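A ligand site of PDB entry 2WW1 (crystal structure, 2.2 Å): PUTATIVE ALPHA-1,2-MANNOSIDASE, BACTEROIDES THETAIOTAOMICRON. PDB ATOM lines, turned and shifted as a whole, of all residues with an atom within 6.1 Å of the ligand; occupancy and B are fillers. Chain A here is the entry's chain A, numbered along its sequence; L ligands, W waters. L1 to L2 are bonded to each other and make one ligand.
Water W2 lies within hydrogen-bond range of an oxygen (O5) of LG2 L2 (2.7 Å), the side-chain amide oxygen (OD1) of Asn 626 (2.8 Å) and the side-chain carboxylate (OD1) of Asp 625 (3.0 Å).
The side-chain carboxylate (OE1) of Glu 514 sits close to a sulfur (S1) of LIG L1 (3.7 Å). CD1 of Trp 69 touches O4 of LG2 L2, 3.1 Å away. CG1 of Ile 70 touches O5 of LG2 L2, 3.7 Å away. CZ3 of Trp 328 touches O2 of LG2 L2, 3.2 Å away. Cys 374 touches the ligand. CG of Met 375 touches O3 of LG2 L2 (3.6 Å). OE1 of Gln 583 touches O2 of LG2 L2 (3.6 Å). Hydrophobic or aromatic side chains that line the ligand: Trp 69, Ile 70, Trp 328, Trp 366, Met 375 and His 565. 14 residues have an atom within 4 Å of the ligand: Ser 67, Trp 69, Ile 70, Trp 328, Asp 329, Trp 366, Cys 374, Met 375, Glu 514, His 565, Glu 566, Gln 583, Asp 623 and Asp 625.
The side-chain carboxylate of Glu 566 sits at hydrogen-bond distance from an oxygen (O3) of LIG L1 (2.5 Å). The side-chain carboxylate (OD1) of Asp 625 is in hydrogen-bond range of an oxygen (O1) of LG2 L2, at 2.5 Å. OD1 of Asp 329 lies within hydrogen-bond range of O3 of LG2 L2 (2.6 Å). An oxygen (O3) of LIG L1 sits at hydrogen-bond distance from a ring nitrogen (NE2) of His 565, at 2.7 Å. O5 of LG2 L2 sits at hydrogen-bond distance from OG of Ser 67 (2.7 Å). The side-chain carboxylate of Asp 623 sits at hydrogen-bond distance from an oxygen (O1) of LG2 L2 (2.8 Å). O3 of LG2 L2 lies within hydrogen-bond range of NE1 of Trp 366 (3.1 Å).
A ring nitrogen (NE2) of His 565 lies within hydrogen-bond range of the side-chain carboxylate of Glu 566, at 3.2 Å. The side-chain carboxylate of Glu 566 sits close to the side-chain carboxylate of Glu 514, 2.7 Å away. The side-chain amide nitrogen of Gln 583 is in hydrogen-bond range of the side-chain carboxylate of Asp 625. The side-chain carboxylate (OD2) of Asp 329 sits close to the side-chain amide oxygen (OE1) of Gln 583, at 3.5 Å. The side-chain hydroxyl (OG) of Ser 67 lies close to the backbone NH (N) of Trp 69. The side-chain hydroxyl of Ser 67 is in hydrogen-bond range of the backbone NH of Ile 70. The side-chain carboxylate (OD2) of Asp 623 sits at hydrogen-bond distance from the indole nitrogen (NE1) of Trp 69.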
ATOM      1  N   PRO A  66       7.180 -33.082 -19.204  1.00  0.00           N
ATOM      2  CA  PRO A  66       8.220 -32.062 -19.086  1.00  0.00           C
ATOM      3  C   PRO A  66       7.909 -30.981 -18.018  1.00  0.00           C
ATOM      4  O   PRO A  66       8.840 -30.364 -17.481  1.00  0.00           O
ATOM      5  CB  PRO A  66       8.222 -31.409 -20.480  1.00  0.00           C
ATOM      6  CG  PRO A  66       6.819 -31.566 -20.962  1.00  0.00           C
ATOM      7  CD  PRO A  66       6.238 -32.805 -20.310  1.00  0.00           C
ATOM      8  N   SER A  67       6.635 -30.772 -17.713  1.00  0.00           N
ATOM      9  CA  SER A  67       6.255 -29.816 -16.670  1.00  0.00           C
ATOM     10  C   SER A  67       4.796 -30.040 -16.323  1.00  0.00           C
ATOM     11  O   SER A  67       4.054 -30.627 -17.110  1.00  0.00           O
ATOM     12  CB  SER A  67       6.431 -28.369 -17.154  1.00  0.00           C
ATOM     13  OG  SER A  67       5.336 -28.054 -17.991  1.00  0.00           O
ATOM     14  N   PRO A  68       4.386 -29.543 -15.161  1.00  0.00           N
ATOM     15  CA  PRO A  68       2.994 -29.711 -14.753  1.00  0.00           C
ATOM     16  C   PRO A  68       2.017 -28.946 -15.655  1.00  0.00           C
ATOM     17  O   PRO A  68       0.857 -29.340 -15.766  1.00  0.00           O
ATOM     18  CB  PRO A  68       2.966 -29.113 -13.336  1.00  0.00           C
ATOM     19  CG  PRO A  68       4.124 -28.128 -13.321  1.00  0.00           C
ATOM     20  CD  PRO A  68       5.185 -28.837 -14.131  1.00  0.00           C
ATOM     21  N   TRP A  69       2.481 -27.854 -16.281  1.00  0.00           N
ATOM     22  CA  TRP A  69       1.603 -27.116 -17.188  1.00  0.00           C
ATOM     23  C   TRP A  69       1.345 -27.898 -18.481  1.00  0.00           C
ATOM     24  O   TRP A  69       0.218 -27.955 -18.982  1.00  0.00           O
ATOM     25  CB  TRP A  69       2.212 -25.738 -17.498  1.00  0.00           C
ATOM     26  CG  TRP A  69       2.792 -25.162 -16.247  1.00  0.00           C
ATOM     27  CD1 TRP A  69       4.111 -25.103 -15.910  1.00  0.00           C
ATOM     28  CD2 TRP A  69       2.054 -24.639 -15.143  1.00  0.00           C
ATOM     29  NE1 TRP A  69       4.240 -24.543 -14.664  1.00  0.00           N
ATOM     30  CE2 TRP A  69       2.997 -24.266 -14.159  1.00  0.00           C
ATOM     31  CE3 TRP A  69       0.689 -24.434 -14.892  1.00  0.00           C
ATOM     32  CZ2 TRP A  69       2.617 -23.707 -12.953  1.00  0.00           C
ATOM     33  CZ3 TRP A  69       0.314 -23.869 -13.692  1.00  0.00           C
ATOM     34  CH2 TRP A  69       1.278 -23.524 -12.731  1.00  0.00           C
ATOM     35  N   ILE A  70       2.392 -28.504 -19.016  1.00  0.00           N
ATOM     36  CA  ILE A  70       2.284 -29.214 -20.262  1.00  0.00           C
ATOM     37  C   ILE A  70       1.619 -30.555 -19.997  1.00  0.00           C
ATOM     38  O   ILE A  70       0.861 -31.052 -20.838  1.00  0.00           O
ATOM     39  CB  ILE A  70       3.646 -29.375 -20.915  1.00  0.00           C
ATOM     40  CG1 ILE A  70       4.157 -27.996 -21.337  1.00  0.00           C
ATOM     41  CG2 ILE A  70       3.614 -30.340 -22.095  1.00  0.00           C
ATOM     42  CD1 ILE A  70       3.408 -27.401 -22.502  1.00  0.00           C
ATOM     43  N   GLY A 326      10.640 -26.874 -24.710  1.00  0.00           N
ATOM     44  CA  GLY A 326      10.181 -25.630 -25.292  1.00  0.00           C
ATOM     45  C   GLY A 326      11.399 -24.738 -25.505  1.00  0.00           C
ATOM     46  O   GLY A 326      12.095 -24.382 -24.550  1.00  0.00           O
ATOM     47  N   TRP A 328      11.621 -21.693 -26.210  1.00  0.00           N
ATOM     48  CA  TRP A 328      11.488 -20.393 -25.522  1.00  0.00           C
ATOM     49  C   TRP A 328      12.257 -20.440 -24.195  1.00  0.00           C
ATOM     50  O   TRP A 328      12.828 -19.422 -23.793  1.00  0.00           O
ATOM     51  CB  TRP A 328      10.015 -20.037 -25.279  1.00  0.00           C
ATOM     52  CG  TRP A 328       9.818 -18.699 -24.608  1.00  0.00           C
ATOM     53  CD1 TRP A 328       9.660 -17.483 -25.219  1.00  0.00           C
ATOM     54  CD2 TRP A 328       9.741 -18.443 -23.194  1.00  0.00           C
ATOM     55  NE1 TRP A 328       9.498 -16.485 -24.267  1.00  0.00           N
ATOM     56  CE2 TRP A 328       9.562 -17.049 -23.018  1.00  0.00           C
ATOM     57  CE3 TRP A 328       9.814 -19.258 -22.065  1.00  0.00           C
ATOM     58  CZ2 TRP A 328       9.459 -16.447 -21.758  1.00  0.00           C
ATOM     59  CZ3 TRP A 328       9.714 -18.672 -20.800  1.00  0.00           C
ATOM     60  CH2 TRP A 328       9.526 -17.266 -20.658  1.00  0.00           C
ATOM     61  N   ASP A 329      12.262 -21.584 -23.521  1.00  0.00           N
ATOM     62  CA  ASP A 329      13.101 -21.784 -22.326  1.00  0.00           C
ATOM     63  C   ASP A 329      14.550 -22.063 -22.740  1.00  0.00           C
ATOM     64  O   ASP A 329      15.451 -21.385 -22.322  1.00  0.00           O
ATOM     65  CB  ASP A 329      12.643 -22.987 -21.474  1.00  0.00           C
ATOM     66  CG  ASP A 329      11.244 -22.810 -20.867  1.00  0.00           C
ATOM     67  OD1 ASP A 329      10.370 -23.703 -21.068  1.00  0.00           O
ATOM     68  OD2 ASP A 329      11.020 -21.785 -20.181  1.00  0.00           O
ATOM     69  N   TRP A 366       7.504 -25.338 -28.938  1.00  0.00           N
ATOM     70  CA  TRP A 366       7.176 -26.274 -27.864  1.00  0.00           C
ATOM     71  C   TRP A 366       6.695 -27.576 -28.472  1.00  0.00           C
ATOM     72  O   TRP A 366       5.771 -27.590 -29.285  1.00  0.00           O
ATOM     73  CB  TRP A 366       6.100 -25.731 -26.928  1.00  0.00           C
ATOM     74  CG  TRP A 366       6.603 -25.487 -25.554  1.00  0.00           C
ATOM     75  CD1 TRP A 366       6.759 -24.290 -24.933  1.00  0.00           C
ATOM     76  CD2 TRP A 366       7.033 -26.484 -24.621  1.00  0.00           C
ATOM     77  NE1 TRP A 366       7.245 -24.470 -23.665  1.00  0.00           N
ATOM     78  CE2 TRP A 366       7.425 -25.816 -23.440  1.00  0.00           C
ATOM     79  CE3 TRP A 366       7.125 -27.891 -24.673  1.00  0.00           C
ATOM     80  CZ2 TRP A 366       7.902 -26.486 -22.337  1.00  0.00           C
ATOM     81  CZ3 TRP A 366       7.602 -28.561 -23.570  1.00  0.00           C
ATOM     82  CH2 TRP A 366       7.980 -27.858 -22.405  1.00  0.00           C
ATOM     83  N   CYS A 374       2.233 -23.157 -26.608  1.00  0.00           N
ATOM     84  CA  CYS A 374       2.749 -22.665 -25.333  1.00  0.00           C
ATOM     85  C   CYS A 374       3.936 -21.751 -25.616  1.00  0.00           C
ATOM     86  O   CYS A 374       4.831 -22.127 -26.387  1.00  0.00           O
ATOM     87  CB  CYS A 374       3.243 -23.866 -24.500  1.00  0.00           C
ATOM     88  SG  CYS A 374       3.633 -23.455 -22.827  1.00  0.00           S
ATOM     89  N   MET A 375       3.945 -20.579 -24.988  1.00  0.00           N
ATOM     90  CA  MET A 375       5.014 -19.603 -25.103  1.00  0.00           C
ATOM     91  C   MET A 375       5.077 -18.926 -26.495  1.00  0.00           C
ATOM     92  O   MET A 375       4.100 -18.941 -27.222  1.00  0.00           O
ATOM     93  CB  MET A 375       6.379 -20.145 -24.611  1.00  0.00           C
ATOM     94  CG  MET A 375       6.379 -20.776 -23.227  1.00  0.00           C
ATOM     95  SD  MET A 375       5.511 -19.789 -21.961  1.00  0.00           S
ATOM     96  CE  MET A 375       6.502 -18.329 -22.057  1.00  0.00           C
ATOM     97  N   GLU A 514       5.453 -13.737 -19.574  1.00  0.00           N
ATOM     98  CA  GLU A 514       6.035 -14.152 -18.290  1.00  0.00           C
ATOM     99  C   GLU A 514       6.833 -13.046 -17.625  1.00  0.00           C
ATOM    100  O   GLU A 514       7.856 -13.297 -16.989  1.00  0.00           O
ATOM    101  CB  GLU A 514       6.946 -15.380 -18.478  1.00  0.00           C
ATOM    102  CG  GLU A 514       6.232 -16.576 -18.989  1.00  0.00           C
ATOM    103  CD  GLU A 514       5.626 -17.417 -17.882  1.00  0.00           C
ATOM    104  OE1 GLU A 514       4.387 -17.464 -17.801  1.00  0.00           O
ATOM    105  OE2 GLU A 514       6.407 -18.004 -17.098  1.00  0.00           O
ATOM    106  N   TYR A 560      -3.635 -11.365 -16.052  1.00  0.00           N
ATOM    107  CA  TYR A 560      -3.872 -12.750 -15.630  1.00  0.00           C
ATOM    108  C   TYR A 560      -5.109 -12.935 -14.746  1.00  0.00           C
ATOM    109  O   TYR A 560      -5.650 -14.032 -14.677  1.00  0.00           O
ATOM    110  CB  TYR A 560      -2.658 -13.333 -14.912  1.00  0.00           C
ATOM    111  CG  TYR A 560      -1.401 -13.301 -15.727  1.00  0.00           C
ATOM    112  CD1 TYR A 560      -1.137 -14.304 -16.677  1.00  0.00           C
ATOM    113  CD2 TYR A 560      -0.487 -12.269 -15.577  1.00  0.00           C
ATOM    114  CE1 TYR A 560       0.005 -14.279 -17.432  1.00  0.00           C
ATOM    115  CE2 TYR A 560       0.667 -12.233 -16.343  1.00  0.00           C
ATOM    116  CZ  TYR A 560       0.903 -13.243 -17.259  1.00  0.00           C
ATOM    117  OH  TYR A 560       2.056 -13.208 -18.007  1.00  0.00           O
ATOM    118  N   ILE A 564      -0.193 -14.879 -10.329  1.00  0.00           N
ATOM    119  CA  ILE A 564       0.386 -16.136 -10.768  1.00  0.00           C
ATOM    120  C   ILE A 564       1.710 -16.390 -10.063  1.00  0.00           C
ATOM    121  O   ILE A 564       2.362 -15.471  -9.576  1.00  0.00           O
ATOM    122  CB  ILE A 564       0.607 -16.189 -12.303  1.00  0.00           C
ATOM    123  CG1 ILE A 564       1.468 -15.011 -12.767  1.00  0.00           C
ATOM    124  CG2 ILE A 564      -0.735 -16.213 -13.021  1.00  0.00           C
ATOM    125  CD1 ILE A 564       1.837 -15.050 -14.246  1.00  0.00           C
ATOM    126  N   HIS A 565       2.108 -17.647 -10.009  1.00  0.00           N
ATOM    127  CA  HIS A 565       3.280 -17.988  -9.200  1.00  0.00           C
ATOM    128  C   HIS A 565       4.518 -17.205  -9.614  1.00  0.00           C
ATOM    129  O   HIS A 565       5.331 -16.876  -8.774  1.00  0.00           O
ATOM    130  CB  HIS A 565       3.514 -19.509  -9.167  1.00  0.00           C
ATOM    131  CG  HIS A 565       3.845 -20.089 -10.508  1.00  0.00           C
ATOM    132  ND1 HIS A 565       5.146 -20.232 -10.954  1.00  0.00           N
ATOM    133  CD2 HIS A 565       3.054 -20.544 -11.509  1.00  0.00           C
ATOM    134  CE1 HIS A 565       5.134 -20.767 -12.167  1.00  0.00           C
ATOM    135  NE2 HIS A 565       3.877 -20.958 -12.532  1.00  0.00           N
ATOM    136  N   GLU A 566       4.653 -16.880 -10.898  1.00  0.00           N
ATOM    137  CA  GLU A 566       5.859 -16.152 -11.350  1.00  0.00           C
ATOM    138  C   GLU A 566       5.963 -14.767 -10.705  1.00  0.00           C
ATOM    139  O   GLU A 566       7.067 -14.305 -10.350  1.00  0.00           O
ATOM    140  CB  GLU A 566       5.917 -16.029 -12.875  1.00  0.00           C
ATOM    141  CG  GLU A 566       6.213 -17.346 -13.612  1.00  0.00           C
ATOM    142  CD  GLU A 566       4.941 -18.082 -14.058  1.00  0.00           C
ATOM    143  OE1 GLU A 566       3.865 -17.858 -13.471  1.00  0.00           O
ATOM    144  OE2 GLU A 566       5.033 -18.907 -14.987  1.00  0.00           O
ATOM    145  N   GLN A 583      12.614 -16.497 -17.547  1.00  0.00           N
ATOM    146  CA  GLN A 583      13.703 -16.766 -18.518  1.00  0.00           C
ATOM    147  C   GLN A 583      14.248 -15.546 -19.269  1.00  0.00           C
ATOM    148  O   GLN A 583      15.445 -15.439 -19.522  1.00  0.00           O
ATOM    149  CB  GLN A 583      13.298 -17.881 -19.493  1.00  0.00           C
ATOM    150  CG  GLN A 583      13.687 -19.304 -19.047  1.00  0.00           C
ATOM    151  CD  GLN A 583      12.892 -19.778 -17.836  1.00  0.00           C
ATOM    152  OE1 GLN A 583      11.715 -19.444 -17.697  1.00  0.00           O
ATOM    153  NE2 GLN A 583      13.538 -20.540 -16.947  1.00  0.00           N
ATOM    154  N   ASP A 623      10.226 -22.223 -11.720  1.00  0.00           N
ATOM    155  CA  ASP A 623      10.257 -23.410 -12.613  1.00  0.00           C
ATOM    156  C   ASP A 623      11.645 -23.805 -13.126  1.00  0.00           C
ATOM    157  O   ASP A 623      12.368 -22.989 -13.642  1.00  0.00           O
ATOM    158  CB  ASP A 623       9.298 -23.221 -13.811  1.00  0.00           C
ATOM    159  CG  ASP A 623       7.834 -23.460 -13.431  1.00  0.00           C
ATOM    160  OD1 ASP A 623       7.570 -23.801 -12.260  1.00  0.00           O
ATOM    161  OD2 ASP A 623       6.946 -23.311 -14.293  1.00  0.00           O
ATOM    162  N   ASP A 625      12.191 -25.685 -15.742  1.00  0.00           N
ATOM    163  CA  ASP A 625      12.076 -25.572 -17.202  1.00  0.00           C
ATOM    164  C   ASP A 625      13.037 -26.432 -18.044  1.00  0.00           C
ATOM    165  O   ASP A 625      13.764 -25.922 -18.909  1.00  0.00           O
ATOM    166  CB  ASP A 625      12.188 -24.099 -17.623  1.00  0.00           C
ATOM    167  CG  ASP A 625      11.008 -23.280 -17.135  1.00  0.00           C
ATOM    168  OD1 ASP A 625       9.851 -23.717 -17.323  1.00  0.00           O
ATOM    169  OD2 ASP A 625      11.229 -22.204 -16.524  1.00  0.00           O
ATOM    170  N   ASN A 626      13.043 -27.743 -17.782  1.00  0.00           N
ATOM    171  CA  ASN A 626      13.684 -28.692 -18.681  1.00  0.00           C
ATOM    172  C   ASN A 626      15.183 -28.435 -18.926  1.00  0.00           C
ATOM    173  O   ASN A 626      15.686 -28.628 -20.057  1.00  0.00           O
ATOM    174  CB  ASN A 626      12.887 -28.725 -19.994  1.00  0.00           C
ATOM    175  CG  ASN A 626      11.405 -28.967 -19.730  1.00  0.00           C
ATOM    176  OD1 ASN A 626      10.553 -28.154 -20.067  1.00  0.00           O
ATOM    177  ND2 ASN A 626      11.125 -30.087 -19.067  1.00  0.00           N
HETATM  178  S1  LIG L   1       4.232 -21.108 -18.155  1.00  0.00           S
HETATM  179  C1  LIG L   1       2.714 -21.695 -17.328  1.00  0.00           C
HETATM  180  C2  LIG L   1       1.526 -21.374 -18.230  1.00  0.00           C
HETATM  181  O1  LIG L   1       0.545 -22.100 -17.589  1.00  0.00           O
HETATM  182  C3  LIG L   1      -0.515 -22.209 -18.564  1.00  0.00           C
HETATM  183  O2  LIG L   1       0.941 -20.057 -18.199  1.00  0.00           O
HETATM  184  C4  LIG L   1       2.540 -21.121 -15.903  1.00  0.00           C
HETATM  185  O3  LIG L   1       3.787 -21.087 -15.193  1.00  0.00           O
HETATM  186  C5  LIG L   1       1.942 -19.718 -16.019  1.00  0.00           C
HETATM  187  O4  LIG L   1       1.704 -19.206 -14.713  1.00  0.00           O
HETATM  188  C6  LIG L   1       0.654 -19.776 -16.875  1.00  0.00           C
HETATM  189  C7  LIG L   1       0.215 -18.337 -16.992  1.00  0.00           C
HETATM  190  O5  LIG L   1      -0.881 -18.303 -17.881  1.00  0.00           O
HETATM  191  C1  LG2 L   2       5.446 -22.280 -17.507  1.00  0.00           C
HETATM  192  C2  LG2 L   2       6.841 -21.649 -17.618  1.00  0.00           C
HETATM  193  C3  LG2 L   2       7.396 -21.658 -19.034  1.00  0.00           C
HETATM  194  C4  LG2 L   2       7.304 -23.082 -19.593  1.00  0.00           C
HETATM  195  C5  LG2 L   2       5.839 -23.482 -19.567  1.00  0.00           C
HETATM  196  C6  LG2 L   2       5.687 -24.892 -20.144  1.00  0.00           C
HETATM  197  O1  LG2 L   2       7.784 -22.340 -16.772  1.00  0.00           O
HETATM  198  O2  LG2 L   2       8.753 -21.158 -18.955  1.00  0.00           O
HETATM  199  O3  LG2 L   2       7.786 -23.129 -20.949  1.00  0.00           O
HETATM  200  O4  LG2 L   2       5.314 -23.472 -18.225  1.00  0.00           O
HETATM  201  O5  LG2 L   2       6.294 -25.864 -19.276  1.00  0.00           O
HETATM  202  O   HOH W   1      -1.547 -16.587 -19.881  1.00  0.00           O
HETATM  203  O   HOH W   2       8.959 -26.100 -18.934  1.00  0.00           O
HETATM  204  O   HOH W   3      -0.423 -20.028 -13.193  1.00  0.00           O
HETATM  205  O   HOH W   4      -3.121 -19.195 -16.730  1.00  0.00           O
